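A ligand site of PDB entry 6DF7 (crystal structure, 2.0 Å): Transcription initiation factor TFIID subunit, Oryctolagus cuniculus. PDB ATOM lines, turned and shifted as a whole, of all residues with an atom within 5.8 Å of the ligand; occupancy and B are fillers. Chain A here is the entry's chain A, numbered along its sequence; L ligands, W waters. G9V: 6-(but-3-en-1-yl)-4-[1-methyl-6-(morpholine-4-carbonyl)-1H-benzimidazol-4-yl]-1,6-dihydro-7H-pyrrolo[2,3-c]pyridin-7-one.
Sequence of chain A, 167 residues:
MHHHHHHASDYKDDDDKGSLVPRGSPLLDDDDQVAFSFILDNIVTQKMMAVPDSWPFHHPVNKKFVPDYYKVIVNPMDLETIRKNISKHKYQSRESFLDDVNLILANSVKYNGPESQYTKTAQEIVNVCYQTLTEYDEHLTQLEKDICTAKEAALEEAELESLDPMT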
ATOM      1  N   TRP A  55      -0.062 -29.278  13.012  1.00  0.00           N
ATOM      2  CA  TRP A  55       0.661 -28.918  11.793  1.00  0.00           C
ATOM      3  C   TRP A  55       1.734 -27.816  12.002  1.00  0.00           C
ATOM      4  O   TRP A  55       2.786 -27.952  11.386  1.00  0.00           O
ATOM      5  CB  TRP A  55      -0.297 -28.548  10.601  1.00  0.00           C
ATOM      6  CG  TRP A  55      -1.124 -27.323  10.846  1.00  0.00           C
ATOM      7  CD1 TRP A  55      -2.352 -27.277  11.441  1.00  0.00           C
ATOM      8  CD2 TRP A  55      -0.709 -25.961  10.651  1.00  0.00           C
ATOM      9  NE1 TRP A  55      -2.720 -25.960  11.646  1.00  0.00           N
ATOM     10  CE2 TRP A  55      -1.739 -25.134  11.163  1.00  0.00           C
ATOM     11  CE3 TRP A  55       0.432 -25.360  10.118  1.00  0.00           C
ATOM     12  CZ2 TRP A  55      -1.652 -23.747  11.149  1.00  0.00           C
ATOM     13  CZ3 TRP A  55       0.523 -23.976  10.117  1.00  0.00           C
ATOM     14  CH2 TRP A  55      -0.500 -23.183  10.642  1.00  0.00           C
ATOM     15  N   PRO A  56       1.573 -26.755  12.874  1.00  0.00           N
ATOM     16  CA  PRO A  56       2.653 -25.739  12.978  1.00  0.00           C
ATOM     17  C   PRO A  56       3.946 -26.289  13.580  1.00  0.00           C
ATOM     18  O   PRO A  56       4.974 -25.667  13.419  1.00  0.00           O
ATOM     19  CB  PRO A  56       2.049 -24.658  13.886  1.00  0.00           C
ATOM     20  CG  PRO A  56       0.579 -24.898  13.878  1.00  0.00           C
ATOM     21  CD  PRO A  56       0.439 -26.385  13.751  1.00  0.00           C
ATOM     22  N   PHE A  57       3.886 -27.479  14.208  1.00  0.00           N
ATOM     23  CA  PHE A  57       5.019 -28.112  14.885  1.00  0.00           C
ATOM     24  C   PHE A  57       5.673 -29.205  14.057  1.00  0.00           C
ATOM     25  O   PHE A  57       6.682 -29.762  14.488  1.00  0.00           O
ATOM     26  CB  PHE A  57       4.541 -28.672  16.252  1.00  0.00           C
ATOM     27  CG  PHE A  57       3.948 -27.600  17.162  1.00  0.00           C
ATOM     28  CD1 PHE A  57       4.783 -26.792  17.940  1.00  0.00           C
ATOM     29  CD2 PHE A  57       2.581 -27.352  17.185  1.00  0.00           C
ATOM     30  CE1 PHE A  57       4.250 -25.782  18.747  1.00  0.00           C
ATOM     31  CE2 PHE A  57       2.040 -26.349  18.008  1.00  0.00           C
ATOM     32  CZ  PHE A  57       2.882 -25.575  18.799  1.00  0.00           C
ATOM     33  N   HIS A  58       5.100 -29.520  12.889  1.00  0.00           N
ATOM     34  CA  HIS A  58       5.605 -30.628  12.063  1.00  0.00           C
ATOM     35  C   HIS A  58       6.917 -30.362  11.391  1.00  0.00           C
ATOM     36  O   HIS A  58       7.650 -31.316  11.130  1.00  0.00           O
ATOM     37  CB  HIS A  58       4.570 -31.059  11.008  1.00  0.00           C
ATOM     38  CG  HIS A  58       3.335 -31.709  11.556  1.00  0.00           C
ATOM     39  ND1 HIS A  58       2.447 -32.368  10.706  1.00  0.00           N
ATOM     40  CD2 HIS A  58       2.861 -31.763  12.816  1.00  0.00           C
ATOM     41  CE1 HIS A  58       1.479 -32.818  11.486  1.00  0.00           C
ATOM     42  NE2 HIS A  58       1.675 -32.465  12.755  1.00  0.00           N
ATOM     43  N   HIS A  59       7.219 -29.102  11.084  1.00  0.00           N
ATOM     44  CA  HIS A  59       8.438 -28.757  10.362  1.00  0.00           C
ATOM     45  C   HIS A  59       9.099 -27.536  10.976  1.00  0.00           C
ATOM     46  O   HIS A  59       8.425 -26.787  11.684  1.00  0.00           O
ATOM     47  CB  HIS A  59       8.104 -28.478   8.873  1.00  0.00           C
ATOM     48  CG  HIS A  59       7.376 -29.591   8.198  1.00  0.00           C
ATOM     49  ND1 HIS A  59       8.040 -30.721   7.755  1.00  0.00           N
ATOM     50  CD2 HIS A  59       6.042 -29.737   7.988  1.00  0.00           C
ATOM     51  CE1 HIS A  59       7.095 -31.513   7.263  1.00  0.00           C
ATOM     52  NE2 HIS A  59       5.883 -30.964   7.374  1.00  0.00           N
ATOM     53  N   PRO A  60      10.408 -27.261  10.666  1.00  0.00           N
ATOM     54  CA  PRO A  60      11.031 -26.029  11.181  1.00  0.00           C
ATOM     55  C   PRO A  60      10.288 -24.796  10.681  1.00  0.00           C
ATOM     56  O   PRO A  60       9.754 -24.771   9.557  1.00  0.00           O
ATOM     57  CB  PRO A  60      12.450 -26.049  10.586  1.00  0.00           C
ATOM     58  CG  PRO A  60      12.661 -27.408  10.067  1.00  0.00           C
ATOM     59  CD  PRO A  60      11.338 -28.029   9.804  1.00  0.00           C
ATOM     60  N   VAL A  61      10.240 -23.760  11.516  1.00  0.00           N
ATOM     61  CA  VAL A  61       9.638 -22.474  11.169  1.00  0.00           C
ATOM     62  C   VAL A  61      10.380 -21.848   9.977  1.00  0.00           C
ATOM     63  O   VAL A  61      11.615 -21.837   9.949  1.00  0.00           O
ATOM     64  CB  VAL A  61       9.664 -21.491  12.380  1.00  0.00           C
ATOM     65  CG1 VAL A  61       9.299 -20.064  11.974  1.00  0.00           C
ATOM     66  CG2 VAL A  61       8.733 -21.973  13.477  1.00  0.00           C
ATOM     67  N   ASN A  62       9.637 -21.325   9.019  1.00  0.00           N
ATOM     68  CA  ASN A  62      10.208 -20.589   7.895  1.00  0.00           C
ATOM     69  C   ASN A  62      10.094 -19.127   8.326  1.00  0.00           C
ATOM     70  O   ASN A  62       8.971 -18.622   8.511  1.00  0.00           O
ATOM     71  CB  ASN A  62       9.383 -20.837   6.616  1.00  0.00           C
ATOM     72  CG  ASN A  62       9.968 -20.230   5.360  1.00  0.00           C
ATOM     73  OD1 ASN A  62      10.628 -19.198   5.353  1.00  0.00           O
ATOM     74  ND2 ASN A  62       9.719 -20.864   4.233  1.00  0.00           N
ATOM     75  N   LYS A  63      11.236 -18.436   8.491  1.00  0.00           N
ATOM     76  CA  LYS A  63      11.229 -17.022   8.920  1.00  0.00           C
ATOM     77  C   LYS A  63      10.490 -16.092   7.934  1.00  0.00           C
ATOM     78  O   LYS A  63      10.081 -15.003   8.332  1.00  0.00           O
ATOM     79  CB  LYS A  63      12.626 -16.484   9.270  1.00  0.00           C
ATOM     80  CG  LYS A  63      13.662 -16.497   8.160  1.00  0.00           C
ATOM     81  CD  LYS A  63      15.020 -16.007   8.673  1.00  0.00           C
ATOM     82  CE  LYS A  63      16.076 -17.093   8.867  1.00  0.00           C
ATOM     83  NZ  LYS A  63      17.203 -16.636   9.729  1.00  0.00           N
ATOM     84  N   PHE A  65       7.473 -16.561   7.068  1.00  0.00           N
ATOM     85  CA  PHE A  65       6.103 -16.495   7.587  1.00  0.00           C
ATOM     86  C   PHE A  65       6.068 -15.980   9.024  1.00  0.00           C
ATOM     87  O   PHE A  65       5.038 -15.474   9.459  1.00  0.00           O
ATOM     88  CB  PHE A  65       5.406 -17.864   7.504  1.00  0.00           C
ATOM     89  CG  PHE A  65       5.394 -18.494   6.127  1.00  0.00           C
ATOM     90  CD1 PHE A  65       4.880 -17.798   5.035  1.00  0.00           C
ATOM     91  CD2 PHE A  65       5.882 -19.773   5.927  1.00  0.00           C
ATOM     92  CE1 PHE A  65       4.877 -18.370   3.759  1.00  0.00           C
ATOM     93  CE2 PHE A  65       5.879 -20.345   4.652  1.00  0.00           C
ATOM     94  CZ  PHE A  65       5.367 -19.643   3.575  1.00  0.00           C
ATOM     95  N   VAL A  66       7.166 -16.176   9.785  1.00  0.00           N
ATOM     96  CA  VAL A  66       7.276 -15.827  11.212  1.00  0.00           C
ATOM     97  C   VAL A  66       8.633 -15.085  11.352  1.00  0.00           C
ATOM     98  O   VAL A  66       9.647 -15.696  11.679  1.00  0.00           O
ATOM     99  CB  VAL A  66       7.133 -17.144  12.055  1.00  0.00           C
ATOM    100  CG1 VAL A  66       7.096 -16.874  13.554  1.00  0.00           C
ATOM    101  CG2 VAL A  66       5.885 -17.936  11.637  1.00  0.00           C
ATOM    102  N   TYR A  69      11.064 -15.184  14.666  1.00  0.00           N
ATOM    103  CA  TYR A  69      11.096 -16.455  15.389  1.00  0.00           C
ATOM    104  C   TYR A  69      12.467 -16.827  15.926  1.00  0.00           C
ATOM    105  O   TYR A  69      12.598 -17.120  17.115  1.00  0.00           O
ATOM    106  CB  TYR A  69      10.515 -17.619  14.576  1.00  0.00           C
ATOM    107  CG  TYR A  69      10.308 -18.856  15.420  1.00  0.00           C
ATOM    108  CD1 TYR A  69       9.216 -18.962  16.272  1.00  0.00           C
ATOM    109  CD2 TYR A  69      11.206 -19.920  15.376  1.00  0.00           C
ATOM    110  CE1 TYR A  69       9.011 -20.094  17.054  1.00  0.00           C
ATOM    111  CE2 TYR A  69      11.025 -21.057  16.156  1.00  0.00           C
ATOM    112  CZ  TYR A  69       9.911 -21.139  16.983  1.00  0.00           C
ATOM    113  OH  TYR A  69       9.710 -22.252  17.775  1.00  0.00           O
ATOM    114  N   MET A  77      13.074 -26.369  17.624  1.00  0.00           N
ATOM    115  CA  MET A  77      12.781 -27.784  17.559  1.00  0.00           C
ATOM    116  C   MET A  77      11.456 -27.972  16.855  1.00  0.00           C
ATOM    117  O   MET A  77      10.571 -27.148  16.995  1.00  0.00           O
ATOM    118  CB  MET A  77      12.780 -28.415  18.981  1.00  0.00           C
ATOM    119  CG  MET A  77      12.774 -29.954  18.995  1.00  0.00           C
ATOM    120  SD  MET A  77      13.982 -30.791  17.946  1.00  0.00           S
ATOM    121  CE  MET A  77      15.540 -30.164  18.595  1.00  0.00           C
ATOM    122  N   ASP A  78      11.309 -29.068  16.135  1.00  0.00           N
ATOM    123  CA  ASP A  78      10.077 -29.446  15.457  1.00  0.00           C
ATOM    124  C   ASP A  78      10.091 -30.958  15.326  1.00  0.00           C
ATOM    125  O   ASP A  78      11.130 -31.589  15.525  1.00  0.00           O
ATOM    126  CB  ASP A  78       9.975 -28.760  14.090  1.00  0.00           C
ATOM    127  CG  ASP A  78      11.044 -29.259  13.161  1.00  0.00           C
ATOM    128  OD1 ASP A  78      12.156 -28.706  13.193  1.00  0.00           O
ATOM    129  OD2 ASP A  78      10.780 -30.241  12.431  1.00  0.00           O
ATOM    130  N   LEU A  79       8.941 -31.529  14.967  1.00  0.00           N
ATOM    131  CA  LEU A  79       8.741 -32.971  14.818  1.00  0.00           C
ATOM    132  C   LEU A  79       9.564 -33.611  13.692  1.00  0.00           C
ATOM    133  O   LEU A  79      10.025 -34.743  13.876  1.00  0.00           O
ATOM    134  CB  LEU A  79       7.248 -33.330  14.723  1.00  0.00           C
ATOM    135  CG  LEU A  79       6.414 -32.866  15.960  1.00  0.00           C
ATOM    136  CD1 LEU A  79       4.963 -33.259  15.836  1.00  0.00           C
ATOM    137  CD2 LEU A  79       6.974 -33.431  17.263  1.00  0.00           C
ATOM    138  N   ILE A 104       9.857 -28.230  22.409  1.00  0.00           N
ATOM    139  CA  ILE A 104       8.686 -27.787  21.619  1.00  0.00           C
ATOM    140  C   ILE A 104       7.706 -26.985  22.506  1.00  0.00           C
ATOM    141  O   ILE A 104       7.270 -25.891  22.114  1.00  0.00           O
ATOM    142  CB  ILE A 104       8.022 -28.990  20.903  1.00  0.00           C
ATOM    143  CG1 ILE A 104       8.906 -29.419  19.695  1.00  0.00           C
ATOM    144  CG2 ILE A 104       6.601 -28.676  20.448  1.00  0.00           C
ATOM    145  CD1 ILE A 104       8.628 -30.774  19.194  1.00  0.00           C
ATOM    146  N   SER A 108       7.317 -22.737  22.578  1.00  0.00           N
ATOM    147  CA  SER A 108       5.993 -22.153  22.407  1.00  0.00           C
ATOM    148  C   SER A 108       5.648 -21.197  23.549  1.00  0.00           C
ATOM    149  O   SER A 108       5.093 -20.135  23.275  1.00  0.00           O
ATOM    150  CB  SER A 108       4.911 -23.220  22.292  1.00  0.00           C
ATOM    151  OG  SER A 108       3.683 -22.589  21.937  1.00  0.00           O
ATOM    152  N   TYR A 111       7.818 -18.044  22.895  1.00  0.00           N
ATOM    153  CA  TYR A 111       7.439 -17.239  21.726  1.00  0.00           C
ATOM    154  C   TYR A 111       5.975 -16.761  21.726  1.00  0.00           C
ATOM    155  O   TYR A 111       5.712 -15.612  21.362  1.00  0.00           O
ATOM    156  CB  TYR A 111       7.775 -17.998  20.423  1.00  0.00           C
ATOM    157  CG  TYR A 111       7.643 -17.119  19.207  1.00  0.00           C
ATOM    158  CD1 TYR A 111       8.620 -16.177  18.903  1.00  0.00           C
ATOM    159  CD2 TYR A 111       6.492 -17.147  18.431  1.00  0.00           C
ATOM    160  CE1 TYR A 111       8.459 -15.287  17.845  1.00  0.00           C
ATOM    161  CE2 TYR A 111       6.325 -16.267  17.365  1.00  0.00           C
ATOM    162  CZ  TYR A 111       7.317 -15.336  17.077  1.00  0.00           C
ATOM    163  OH  TYR A 111       7.146 -14.482  16.022  1.00  0.00           O
ATOM    164  N   ASN A 112       5.035 -17.650  22.059  1.00  0.00           N
ATOM    165  CA  ASN A 112       3.603 -17.379  21.987  1.00  0.00           C
ATOM    166  C   ASN A 112       2.940 -16.957  23.293  1.00  0.00           C
ATOM    167  O   ASN A 112       1.856 -16.391  23.271  1.00  0.00           O
ATOM    168  CB  ASN A 112       2.903 -18.626  21.426  1.00  0.00           C
ATOM    169  CG  ASN A 112       3.430 -19.046  20.076  1.00  0.00           C
ATOM    170  OD1 ASN A 112       3.405 -18.272  19.121  1.00  0.00           O
ATOM    171  ND2 ASN A 112       3.929 -20.254  19.972  1.00  0.00           N
ATOM    172  N   TYR A 118      -1.271 -22.117  20.464  1.00  0.00           N
ATOM    173  CA  TYR A 118      -0.060 -22.860  20.068  1.00  0.00           C
ATOM    174  C   TYR A 118       0.472 -23.630  21.245  1.00  0.00           C
ATOM    175  O   TYR A 118       0.821 -24.797  21.094  1.00  0.00           O
ATOM    176  CB  TYR A 118       1.063 -21.911  19.577  1.00  0.00           C
ATOM    177  CG  TYR A 118       0.805 -21.330  18.218  1.00  0.00           C
ATOM    178  CD1 TYR A 118       1.094 -22.059  17.060  1.00  0.00           C
ATOM    179  CD2 TYR A 118       0.355 -20.013  18.070  1.00  0.00           C
ATOM    180  CE1 TYR A 118       0.847 -21.525  15.794  1.00  0.00           C
ATOM    181  CE2 TYR A 118       0.140 -19.460  16.805  1.00  0.00           C
ATOM    182  CZ  TYR A 118       0.391 -20.231  15.681  1.00  0.00           C
ATOM    183  OH  TYR A 118       0.198 -19.702  14.442  1.00  0.00           O
HETATM  184  C7  G9V L   1       3.587 -20.983   9.333  1.00  0.00           C
HETATM  185  C9  G9V L   1       4.879 -21.555  11.328  1.00  0.00           C
HETATM  186  N2  G9V L   1       1.313 -19.974   9.903  1.00  0.00           N
HETATM  187  C10 G9V L   1       3.864 -21.089  12.162  1.00  0.00           C
HETATM  188  C6  G9V L   1       2.557 -20.528  10.155  1.00  0.00           C
HETATM  189  C29 G9V L   1       4.397 -23.966   8.357  1.00  0.00           C
HETATM  190  N20 G9V L   1       3.798 -18.802  16.458  1.00  0.00           N
HETATM  191  C18 G9V L   1       3.296 -18.634  14.308  1.00  0.00           C
HETATM  192  C11 G9V L   1       4.063 -21.123  13.652  1.00  0.00           C
HETATM  193  C1  G9V L   1       0.744 -19.705   8.578  1.00  0.00           C
HETATM  194  C8  G9V L   1       4.751 -21.506   9.917  1.00  0.00           C
HETATM  195  C16 G9V L   1       4.120 -20.031  15.883  1.00  0.00           C
HETATM  196  C5  G9V L   1       2.672 -20.581  11.570  1.00  0.00           C
HETATM  197  O15 G9V L   1       4.924 -21.300  17.623  1.00  0.00           O
HETATM  198  N13 G9V L   1       4.824 -22.316  15.605  1.00  0.00           N
HETATM  199  C24 G9V L   1       7.530 -24.960  16.191  1.00  0.00           C
HETATM  200  C25 G9V L   1       7.914 -25.872  15.327  1.00  0.00           C
HETATM  201  C32 G9V L   1       6.963 -25.172   7.720  1.00  0.00           C
HETATM  202  C17 G9V L   1       3.806 -19.943  14.514  1.00  0.00           C
HETATM  203  C22 G9V L   1       5.417 -23.578  16.113  1.00  0.00           C
HETATM  204  O31 G9V L   1       5.720 -25.898   7.872  1.00  0.00           O
HETATM  205  C12 G9V L   1       4.552 -22.254  14.247  1.00  0.00           C
HETATM  206  C19 G9V L   1       3.284 -17.974  15.493  1.00  0.00           C
HETATM  207  C14 G9V L   1       4.649 -21.241  16.417  1.00  0.00           C
HETATM  208  N28 G9V L   1       5.651 -23.170   8.300  1.00  0.00           N
HETATM  209  C33 G9V L   1       6.712 -23.682   7.410  1.00  0.00           C
HETATM  210  C3  G9V L   1       0.728 -19.708  11.110  1.00  0.00           C
HETATM  211  C23 G9V L   1       6.911 -23.659  15.746  1.00  0.00           C
HETATM  212  C26 G9V L   1       5.819 -22.030   9.037  1.00  0.00           C
HETATM  213  C30 G9V L   1       4.771 -25.383   8.808  1.00  0.00           C
HETATM  214  O27 G9V L   1       6.881 -21.421   8.983  1.00  0.00           O
HETATM  215  N4  G9V L   1       1.528 -20.078  12.067  1.00  0.00           N
HETATM  216  O   HOH W   1      10.320 -25.357   7.005  1.00  0.00           O
HETATM  217  O   HOH W   2       7.214 -22.282  19.122  1.00  0.00           O
HETATM  218  O   HOH W   3       7.523 -24.863  19.681  1.00  0.00           O
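O of Phe 57 is in hydrogen-bond range of N of Leu 79 (2.9 Å). The side-chain hydroxyl (OG) of Ser 108 sits at hydrogen-bond distance from the side-chain amide nitrogen (ND2) of Asn 112, at 3.1 Å.
The side-chain hydroxyl (OH) of Tyr 118 sits at hydrogen-bond distance from a nitrogen (N4) of the ligand. OD1 of Asn 112 sits at hydrogen-bond distance from N20 of the ligand, 2.7 Å away. N of Asn 62 lies within hydrogen-bond range of O27 of the ligand (2.8 Å).
Trp 55 touches the ligand. Pro 56 touches the ligand (O to C22, 3.4 Å). Phe 57 touches the ligand (CE1 to C22, 3.6 Å). His 59 touches the ligand (CB to O31, 3.7 Å). Pro 60 touches the ligand (O to C32, 3.4 Å). Val 61 touches the ligand (CG2 to C23, 3.4 Å). Phe 65 touches the ligand (CD2 to O27, 3.6 Å). Val 66 touches the ligand. OH of Tyr 69 touches C23 of the ligand (3.7 Å). O of Met 77 touches C25 of the ligand (3.4 Å). Asp 78 touches the ligand. Tyr 111 touches the ligand (CE2 to N20, 3.7 Å). The nearest printed residue that does not touch the ligand is Ser 108 (4.7 Å).
Water W2 lies within hydrogen-bond range of the side-chain hydroxyl (OH) of Tyr 69 (2.8 Å), an oxygen (O15) of the ligand (2.9 Å) and the backbone NH (N) of Ser 108 (3.5 Å).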
